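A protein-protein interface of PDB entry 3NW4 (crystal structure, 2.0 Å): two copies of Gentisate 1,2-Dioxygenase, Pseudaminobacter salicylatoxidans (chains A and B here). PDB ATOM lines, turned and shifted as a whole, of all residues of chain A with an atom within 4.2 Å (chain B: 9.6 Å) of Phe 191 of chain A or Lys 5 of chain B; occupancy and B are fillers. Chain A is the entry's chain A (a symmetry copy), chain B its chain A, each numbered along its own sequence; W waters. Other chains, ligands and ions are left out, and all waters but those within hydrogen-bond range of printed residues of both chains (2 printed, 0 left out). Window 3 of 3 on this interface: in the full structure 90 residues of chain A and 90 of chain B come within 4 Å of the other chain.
O of Thr 12 of chain B sits close to O of Arg 79 of chain A (3.3 Å). The backbone carbonyl oxygen of Ile 48 of chain B is in hydrogen-bond range of the backbone NH of Phe 189 of chain A, 3.0 Å away. N of Ala 14 of chain B lies within hydrogen-bond range of O of Arg 79 of chain A. The backbone carbonyl oxygen of Pro 47 of chain B sits at hydrogen-bond distance from the backbone NH of Phe 189 of chain A, 3.2 Å away.
NH1 of Arg 79 of chain A lies within salt-bridge range of OE1 of Glu 82 of chain A (2.7 Å). A ring nitrogen (NE2) of His 8 of chain B sits at hydrogen-bond distance from the backbone carbonyl oxygen (O) of Met 46 of chain B (2.8 Å). The side-chain hydroxyl (OG) of Ser 10 of chain B lies within hydrogen-bond range of the backbone NH (N) of Asp 7 of chain B, at 3.1 Å. The backbone NH (N) of Glu 9 of chain B lies within hydrogen-bond range of the side-chain carboxylate (OD1) of Asp 7 of chain B (3.0 Å). The guanidinium group (NH2) of Arg 79 of chain A lies within hydrogen-bond range of the backbone carbonyl oxygen (O) of Gly 192 of chain A (2.8 Å). O of Glu 118 of chain A lies within hydrogen-bond range of NH1 of Arg 79 of chain A.
CG2 of Val 11 of chain B touches CG of Arg 79 of chain A (3.3 Å). Gln 13 of chain B touches Arg 79 of chain A. Leu 42 of chain B touches Glu 82 of chain A. His 8 of chain B touches Phe 189 of chain A (CE1 to CD1, 3.96 Å). Phe 189 of chain A touches Met 46 of chain B (CB to O, 3.4 Å). Phe 191 of chain A touches Lys 5 of chain B. Phe 191 of chain A touches Leu 6 of chain B (CD2 to CB, 3.8 Å). O of Asp 7 of chain B touches CE2 of Phe 191 of chain A, at 3.8 Å. Phe 191 of chain A touches His 8 of chain B. Val 11 of chain B touches Phe 191 of chain A.
Of the printed residues of chain B, Glu 82 of chain A touches Leu 42 (3.6 Å). Of the printed residues of chain B, Phe 189 of chain A touches His 8 (3.96 Å), Met 46 (3.4 Å), Pro 47 (3.2 Å) and Ile 48 (3.0 Å). Phe 191 of chain A touches just these residues of chain B: Lys 5 (3.5 Å), Leu 6 (3.8 Å), Asp 7 (3.8 Å), His 8 (3.5 Å) and Val 11 (3.7 Å). No residue of chain B comes within 4 Å of Gly 192 of chain A. Of chain A, only Phe 191 (3.5 Å) comes within 4 Å of Lys 5 of chain B. Printed residues of chain A within 4 Å of Ile 48 of chain B: Phe 189.
Printed residues of chain A that touch a printed residue of chain B: Arg 79, Glu 82, Phe 189 and Phe 191. Hydrophobic or aromatic side chains of chain A that line the printed part of chain B: Phe 189 and Phe 191. Among the printed residues, no Asp or Glu carboxylate lies within 4 Å of a Lys or Arg side-chain nitrogen of the other chain.
No position is printed for both chains. Of the 14 pairs that touch across the chains among the printed residues, none has its exchanged pair printed and touching as well.
Water W2 lies within hydrogen-bond range of NZ of Lys 5 of chain B (2.7 Å) and O of Gly 192 of chain A (3.2 Å). Water W1 lies within hydrogen-bond range of O of Leu 6 of chain B (2.9 Å) and N of Phe 191 of chain A (2.9 Å).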
ATOM      1  N   ARG A  79     -22.711  -7.270  -0.466  1.00  0.00           N
ATOM      2  CA  ARG A  79     -23.448  -6.024  -0.672  1.00  0.00           C
ATOM      3  C   ARG A  79     -24.674  -6.144  -1.600  1.00  0.00           C
ATOM      4  O   ARG A  79     -24.702  -6.959  -2.548  1.00  0.00           O
ATOM      5  CB  ARG A  79     -22.469  -4.962  -1.198  1.00  0.00           C
ATOM      6  CG  ARG A  79     -22.904  -3.519  -0.996  1.00  0.00           C
ATOM      7  CD  ARG A  79     -22.381  -2.939   0.297  1.00  0.00           C
ATOM      8  NE  ARG A  79     -23.210  -3.230   1.475  1.00  0.00           N
ATOM      9  CZ  ARG A  79     -22.962  -2.755   2.695  1.00  0.00           C
ATOM     10  NH1 ARG A  79     -23.778  -3.065   3.704  1.00  0.00           N
ATOM     11  NH2 ARG A  79     -21.890  -1.969   2.921  1.00  0.00           N
ATOM     12  N   GLU A  82     -27.359  -8.044   0.692  1.00  0.00           N
ATOM     13  CA  GLU A  82     -26.990  -7.888   2.136  1.00  0.00           C
ATOM     14  C   GLU A  82     -26.813  -9.155   2.987  1.00  0.00           C
ATOM     15  O   GLU A  82     -25.804  -9.282   3.708  1.00  0.00           O
ATOM     16  CB  GLU A  82     -27.908  -6.869   2.858  1.00  0.00           C
ATOM     17  CG  GLU A  82     -27.841  -5.460   2.253  1.00  0.00           C
ATOM     18  CD  GLU A  82     -26.463  -4.781   2.429  1.00  0.00           C
ATOM     19  OE1 GLU A  82     -26.104  -4.448   3.599  1.00  0.00           O
ATOM     20  OE2 GLU A  82     -25.753  -4.581   1.392  1.00  0.00           O
ATOM     21  N   GLU A 118     -21.953  -4.285   7.079  1.00  0.00           N
ATOM     22  CA  GLU A 118     -22.645  -3.532   8.107  1.00  0.00           C
ATOM     23  C   GLU A 118     -23.688  -2.609   7.483  1.00  0.00           C
ATOM     24  O   GLU A 118     -23.441  -1.955   6.453  1.00  0.00           O
ATOM     25  CB  GLU A 118     -21.660  -2.686   8.927  1.00  0.00           C
ATOM     26  CG  GLU A 118     -20.715  -3.518   9.827  1.00  0.00           C
ATOM     27  CD  GLU A 118     -20.160  -2.730  11.032  1.00  0.00           C
ATOM     28  OE1 GLU A 118     -20.462  -1.506  11.162  1.00  0.00           O
ATOM     29  OE2 GLU A 118     -19.423  -3.343  11.845  1.00  0.00           O
ATOM     30  N   PHE A 189     -33.177   3.194   5.807  1.00  0.00           N
ATOM     31  CA  PHE A 189     -32.093   2.219   5.660  1.00  0.00           C
ATOM     32  C   PHE A 189     -30.794   2.954   5.277  1.00  0.00           C
ATOM     33  O   PHE A 189     -30.832   3.916   4.483  1.00  0.00           O
ATOM     34  CB  PHE A 189     -32.443   1.201   4.576  1.00  0.00           C
ATOM     35  CG  PHE A 189     -31.374   0.154   4.346  1.00  0.00           C
ATOM     36  CD1 PHE A 189     -30.207   0.465   3.611  1.00  0.00           C
ATOM     37  CD2 PHE A 189     -31.518  -1.140   4.872  1.00  0.00           C
ATOM     38  CE1 PHE A 189     -29.194  -0.501   3.394  1.00  0.00           C
ATOM     39  CE2 PHE A 189     -30.506  -2.123   4.671  1.00  0.00           C
ATOM     40  CZ  PHE A 189     -29.336  -1.783   3.919  1.00  0.00           C
ATOM     41  N   GLU A 190     -29.667   2.516   5.854  1.00  0.00           N
ATOM     42  CA  GLU A 190     -28.382   3.124   5.549  1.00  0.00           C
ATOM     43  C   GLU A 190     -27.283   2.043   5.410  1.00  0.00           C
ATOM     44  O   GLU A 190     -27.147   1.172   6.285  1.00  0.00           O
ATOM     45  CB  GLU A 190     -28.046   4.195   6.603  1.00  0.00           C
ATOM     46  CG  GLU A 190     -26.781   4.958   6.329  1.00  0.00           C
ATOM     47  CD  GLU A 190     -26.382   5.881   7.463  1.00  0.00           C
ATOM     48  OE1 GLU A 190     -25.154   6.150   7.533  1.00  0.00           O
ATOM     49  OE2 GLU A 190     -27.262   6.331   8.269  1.00  0.00           O
ATOM     50  N   PHE A 191     -26.557   2.046   4.282  1.00  0.00           N
ATOM     51  CA  PHE A 191     -25.425   1.115   4.097  1.00  0.00           C
ATOM     52  C   PHE A 191     -24.283   1.590   4.981  1.00  0.00           C
ATOM     53  O   PHE A 191     -24.035   2.799   5.063  1.00  0.00           O
ATOM     54  CB  PHE A 191     -24.957   1.040   2.620  1.00  0.00           C
ATOM     55  CG  PHE A 191     -25.971   0.439   1.685  1.00  0.00           C
ATOM     56  CD1 PHE A 191     -26.063  -0.923   1.532  1.00  0.00           C
ATOM     57  CD2 PHE A 191     -26.840   1.252   0.954  1.00  0.00           C
ATOM     58  CE1 PHE A 191     -27.004  -1.494   0.652  1.00  0.00           C
ATOM     59  CE2 PHE A 191     -27.769   0.706   0.103  1.00  0.00           C
ATOM     60  CZ  PHE A 191     -27.863  -0.668  -0.059  1.00  0.00           C
ATOM     61  N   GLY A 192     -23.620   0.659   5.672  1.00  0.00           N
ATOM     62  CA  GLY A 192     -22.429   0.997   6.463  1.00  0.00           C
ATOM     63  C   GLY A 192     -21.188   0.401   5.813  1.00  0.00           C
ATOM     64  O   GLY A 192     -21.136   0.183   4.598  1.00  0.00           O
ATOM     65  N   LYS B   5     -24.249   9.431  -0.059  1.00  0.00           N
ATOM     66  CA  LYS B   5     -24.415   8.061   0.515  1.00  0.00           C
ATOM     67  C   LYS B   5     -25.126   7.174  -0.520  1.00  0.00           C
ATOM     68  O   LYS B   5     -25.950   7.658  -1.302  1.00  0.00           O
ATOM     69  CB  LYS B   5     -25.181   8.140   1.853  1.00  0.00           C
ATOM     70  CG  LYS B   5     -25.033   6.963   2.861  1.00  0.00           C
ATOM     71  CD  LYS B   5     -23.588   6.362   3.008  1.00  0.00           C
ATOM     72  CE  LYS B   5     -23.485   4.965   2.313  1.00  0.00           C
ATOM     73  NZ  LYS B   5     -22.100   4.367   2.160  1.00  0.00           N
ATOM     74  N   LEU B   6     -24.776   5.888  -0.532  1.00  0.00           N
ATOM     75  CA  LEU B   6     -25.372   4.909  -1.442  1.00  0.00           C
ATOM     76  C   LEU B   6     -26.878   4.763  -1.240  1.00  0.00           C
ATOM     77  O   LEU B   6     -27.382   4.893  -0.108  1.00  0.00           O
ATOM     78  CB  LEU B   6     -24.742   3.534  -1.219  1.00  0.00           C
ATOM     79  CG  LEU B   6     -23.231   3.412  -1.382  1.00  0.00           C
ATOM     80  CD1 LEU B   6     -22.731   2.142  -0.698  1.00  0.00           C
ATOM     81  CD2 LEU B   6     -22.837   3.476  -2.863  1.00  0.00           C
ATOM     82  N   ASP B   7     -27.591   4.499  -2.329  1.00  0.00           N
ATOM     83  CA  ASP B   7     -28.971   4.052  -2.219  1.00  0.00           C
ATOM     84  C   ASP B   7     -29.098   2.698  -2.934  1.00  0.00           C
ATOM     85  O   ASP B   7     -28.068   2.134  -3.376  1.00  0.00           O
ATOM     86  CB  ASP B   7     -29.962   5.122  -2.720  1.00  0.00           C
ATOM     87  CG  ASP B   7     -29.705   5.559  -4.172  1.00  0.00           C
ATOM     88  OD1 ASP B   7     -29.293   4.712  -5.010  1.00  0.00           O
ATOM     89  OD2 ASP B   7     -29.952   6.759  -4.462  1.00  0.00           O
ATOM     90  N   HIS B   8     -30.319   2.165  -3.034  1.00  0.00           N
ATOM     91  CA  HIS B   8     -30.504   0.823  -3.604  1.00  0.00           C
ATOM     92  C   HIS B   8     -30.209   0.763  -5.123  1.00  0.00           C
ATOM     93  O   HIS B   8     -30.008  -0.322  -5.685  1.00  0.00           O
ATOM     94  CB  HIS B   8     -31.884   0.234  -3.249  1.00  0.00           C
ATOM     95  CG  HIS B   8     -32.053  -0.037  -1.778  1.00  0.00           C
ATOM     96  ND1 HIS B   8     -31.241  -0.911  -1.084  1.00  0.00           N
ATOM     97  CD2 HIS B   8     -32.935   0.453  -0.873  1.00  0.00           C
ATOM     98  CE1 HIS B   8     -31.612  -0.945   0.184  1.00  0.00           C
ATOM     99  NE2 HIS B   8     -32.638  -0.127   0.338  1.00  0.00           N
ATOM    100  N   GLU B   9     -30.176   1.936  -5.758  1.00  0.00           N
ATOM    101  CA  GLU B   9     -29.929   2.038  -7.196  1.00  0.00           C
ATOM    102  C   GLU B   9     -28.442   2.136  -7.505  1.00  0.00           C
ATOM    103  O   GLU B   9     -28.024   1.767  -8.586  1.00  0.00           O
ATOM    104  CB  GLU B   9     -30.684   3.228  -7.821  1.00  0.00           C
ATOM    105  CG  GLU B   9     -32.185   2.990  -7.981  1.00  0.00           C
ATOM    106  CD  GLU B   9     -32.926   2.887  -6.627  1.00  0.00           C
ATOM    107  OE1 GLU B   9     -33.692   1.902  -6.439  1.00  0.00           O
ATOM    108  OE2 GLU B   9     -32.724   3.773  -5.750  1.00  0.00           O
ATOM    109  N   SER B  10     -27.647   2.610  -6.553  1.00  0.00           N
ATOM    110  CA  SER B  10     -26.261   2.908  -6.820  1.00  0.00           C
ATOM    111  C   SER B  10     -25.316   1.924  -6.157  1.00  0.00           C
ATOM    112  O   SER B  10     -24.125   1.915  -6.475  1.00  0.00           O
ATOM    113  CB  SER B  10     -25.934   4.348  -6.390  1.00  0.00           C
ATOM    114  OG  SER B  10     -26.067   4.529  -4.984  1.00  0.00           O
ATOM    115  N   VAL B  11     -25.830   1.116  -5.228  1.00  0.00           N
ATOM    116  CA  VAL B  11     -25.018   0.115  -4.510  1.00  0.00           C
ATOM    117  C   VAL B  11     -24.625  -1.040  -5.459  1.00  0.00           C
ATOM    118  O   VAL B  11     -25.347  -1.352  -6.419  1.00  0.00           O
ATOM    119  CB  VAL B  11     -25.788  -0.448  -3.256  1.00  0.00           C
ATOM    120  CG1 VAL B  11     -27.032  -1.263  -3.667  1.00  0.00           C
ATOM    121  CG2 VAL B  11     -24.879  -1.275  -2.354  1.00  0.00           C
ATOM    122  N   THR B  12     -23.484  -1.664  -5.200  1.00  0.00           N
ATOM    123  CA  THR B  12     -23.099  -2.867  -5.922  1.00  0.00           C
ATOM    124  C   THR B  12     -23.999  -4.044  -5.505  1.00  0.00           C
ATOM    125  O   THR B  12     -24.275  -4.252  -4.301  1.00  0.00           O
ATOM    126  CB  THR B  12     -21.623  -3.204  -5.636  1.00  0.00           C
ATOM    127  OG1 THR B  12     -20.828  -2.046  -5.931  1.00  0.00           O
ATOM    128  CG2 THR B  12     -21.132  -4.403  -6.488  1.00  0.00           C
ATOM    129  N   GLN B  13     -24.468  -4.794  -6.501  1.00  0.00           N
ATOM    130  CA  GLN B  13     -25.257  -5.999  -6.255  1.00  0.00           C
ATOM    131  C   GLN B  13     -24.362  -7.235  -6.295  1.00  0.00           C
ATOM    132  O   GLN B  13     -24.179  -7.854  -7.359  1.00  0.00           O
ATOM    133  CB  GLN B  13     -26.426  -6.111  -7.242  1.00  0.00           C
ATOM    134  CG  GLN B  13     -27.487  -5.029  -7.056  1.00  0.00           C
ATOM    135  CD  GLN B  13     -28.143  -5.035  -5.650  1.00  0.00           C
ATOM    136  OE1 GLN B  13     -28.253  -6.080  -4.983  1.00  0.00           O
ATOM    137  NE2 GLN B  13     -28.592  -3.865  -5.213  1.00  0.00           N
ATOM    138  N   ALA B  14     -23.806  -7.576  -5.132  1.00  0.00           N
ATOM    139  CA  ALA B  14     -22.879  -8.703  -4.979  1.00  0.00           C
ATOM    140  C   ALA B  14     -23.516 -10.086  -4.705  1.00  0.00           C
ATOM    141  O   ALA B  14     -22.800 -11.078  -4.547  1.00  0.00           O
ATOM    142  CB  ALA B  14     -21.836  -8.384  -3.892  1.00  0.00           C
ATOM    143  N   LEU B  42     -34.507  -7.107  -1.251  1.00  0.00           N
ATOM    144  CA  LEU B  42     -33.994  -6.218  -0.178  1.00  0.00           C
ATOM    145  C   LEU B  42     -34.467  -4.770  -0.287  1.00  0.00           C
ATOM    146  O   LEU B  42     -35.005  -4.240   0.688  1.00  0.00           O
ATOM    147  CB  LEU B  42     -32.455  -6.263  -0.009  1.00  0.00           C
ATOM    148  CG  LEU B  42     -32.058  -5.543   1.306  1.00  0.00           C
ATOM    149  CD1 LEU B  42     -31.481  -6.499   2.308  1.00  0.00           C
ATOM    150  CD2 LEU B  42     -31.131  -4.373   1.138  1.00  0.00           C
ATOM    151  N   GLY B  43     -34.283  -4.161  -1.464  1.00  0.00           N
ATOM    152  CA  GLY B  43     -34.489  -2.714  -1.667  1.00  0.00           C
ATOM    153  C   GLY B  43     -35.961  -2.321  -1.592  1.00  0.00           C
ATOM    154  O   GLY B  43     -36.322  -1.207  -1.180  1.00  0.00           O
ATOM    155  N   ASP B  44     -36.810  -3.260  -1.985  1.00  0.00           N
ATOM    156  CA  ASP B  44     -38.251  -3.092  -1.877  1.00  0.00           C
ATOM    157  C   ASP B  44     -38.721  -3.110  -0.415  1.00  0.00           C
ATOM    158  O   ASP B  44     -39.526  -2.270   0.019  1.00  0.00           O
ATOM    159  CB  ASP B  44     -38.947  -4.222  -2.642  1.00  0.00           C
ATOM    160  N   MET B  46     -36.942  -2.788   2.300  1.00  0.00           N
ATOM    161  CA  MET B  46     -36.232  -1.900   3.229  1.00  0.00           C
ATOM    162  C   MET B  46     -35.664  -0.652   2.549  1.00  0.00           C
ATOM    163  O   MET B  46     -34.439  -0.525   2.381  1.00  0.00           O
ATOM    164  CB  MET B  46     -35.127  -2.674   3.979  1.00  0.00           C
ATOM    165  CG  MET B  46     -35.621  -3.996   4.615  1.00  0.00           C
ATOM    166  SD  MET B  46     -34.339  -4.847   5.552  1.00  0.00           S
ATOM    167  CE  MET B  46     -34.658  -4.156   7.140  1.00  0.00           C
ATOM    168  N   PRO B  47     -36.555   0.272   2.148  1.00  0.00           N
ATOM    169  CA  PRO B  47     -36.156   1.475   1.425  1.00  0.00           C
ATOM    170  C   PRO B  47     -35.295   2.432   2.270  1.00  0.00           C
ATOM    171  O   PRO B  47     -35.350   2.417   3.522  1.00  0.00           O
ATOM    172  CB  PRO B  47     -37.499   2.149   1.083  1.00  0.00           C
ATOM    173  CG  PRO B  47     -38.444   1.672   2.244  1.00  0.00           C
ATOM    174  CD  PRO B  47     -38.003   0.240   2.457  1.00  0.00           C
ATOM    175  N   ILE B  48     -34.536   3.277   1.570  1.00  0.00           N
ATOM    176  CA  ILE B  48     -33.667   4.260   2.186  1.00  0.00           C
ATOM    177  C   ILE B  48     -34.467   5.218   3.108  1.00  0.00           C
ATOM    178  O   ILE B  48     -34.005   5.595   4.202  1.00  0.00           O
ATOM    179  CB  ILE B  48     -32.899   5.064   1.067  1.00  0.00           C
ATOM    180  CG1 ILE B  48     -32.001   4.131   0.216  1.00  0.00           C
ATOM    181  CG2 ILE B  48     -32.158   6.280   1.658  1.00  0.00           C
ATOM    182  CD1 ILE B  48     -30.875   3.421   0.938  1.00  0.00           C
HETATM  183  O   HOH W   1     -26.573   4.426   2.614  1.00  0.00           O
HETATM  184  O   HOH W   2     -20.591   2.089   2.034  1.00  0.00           O
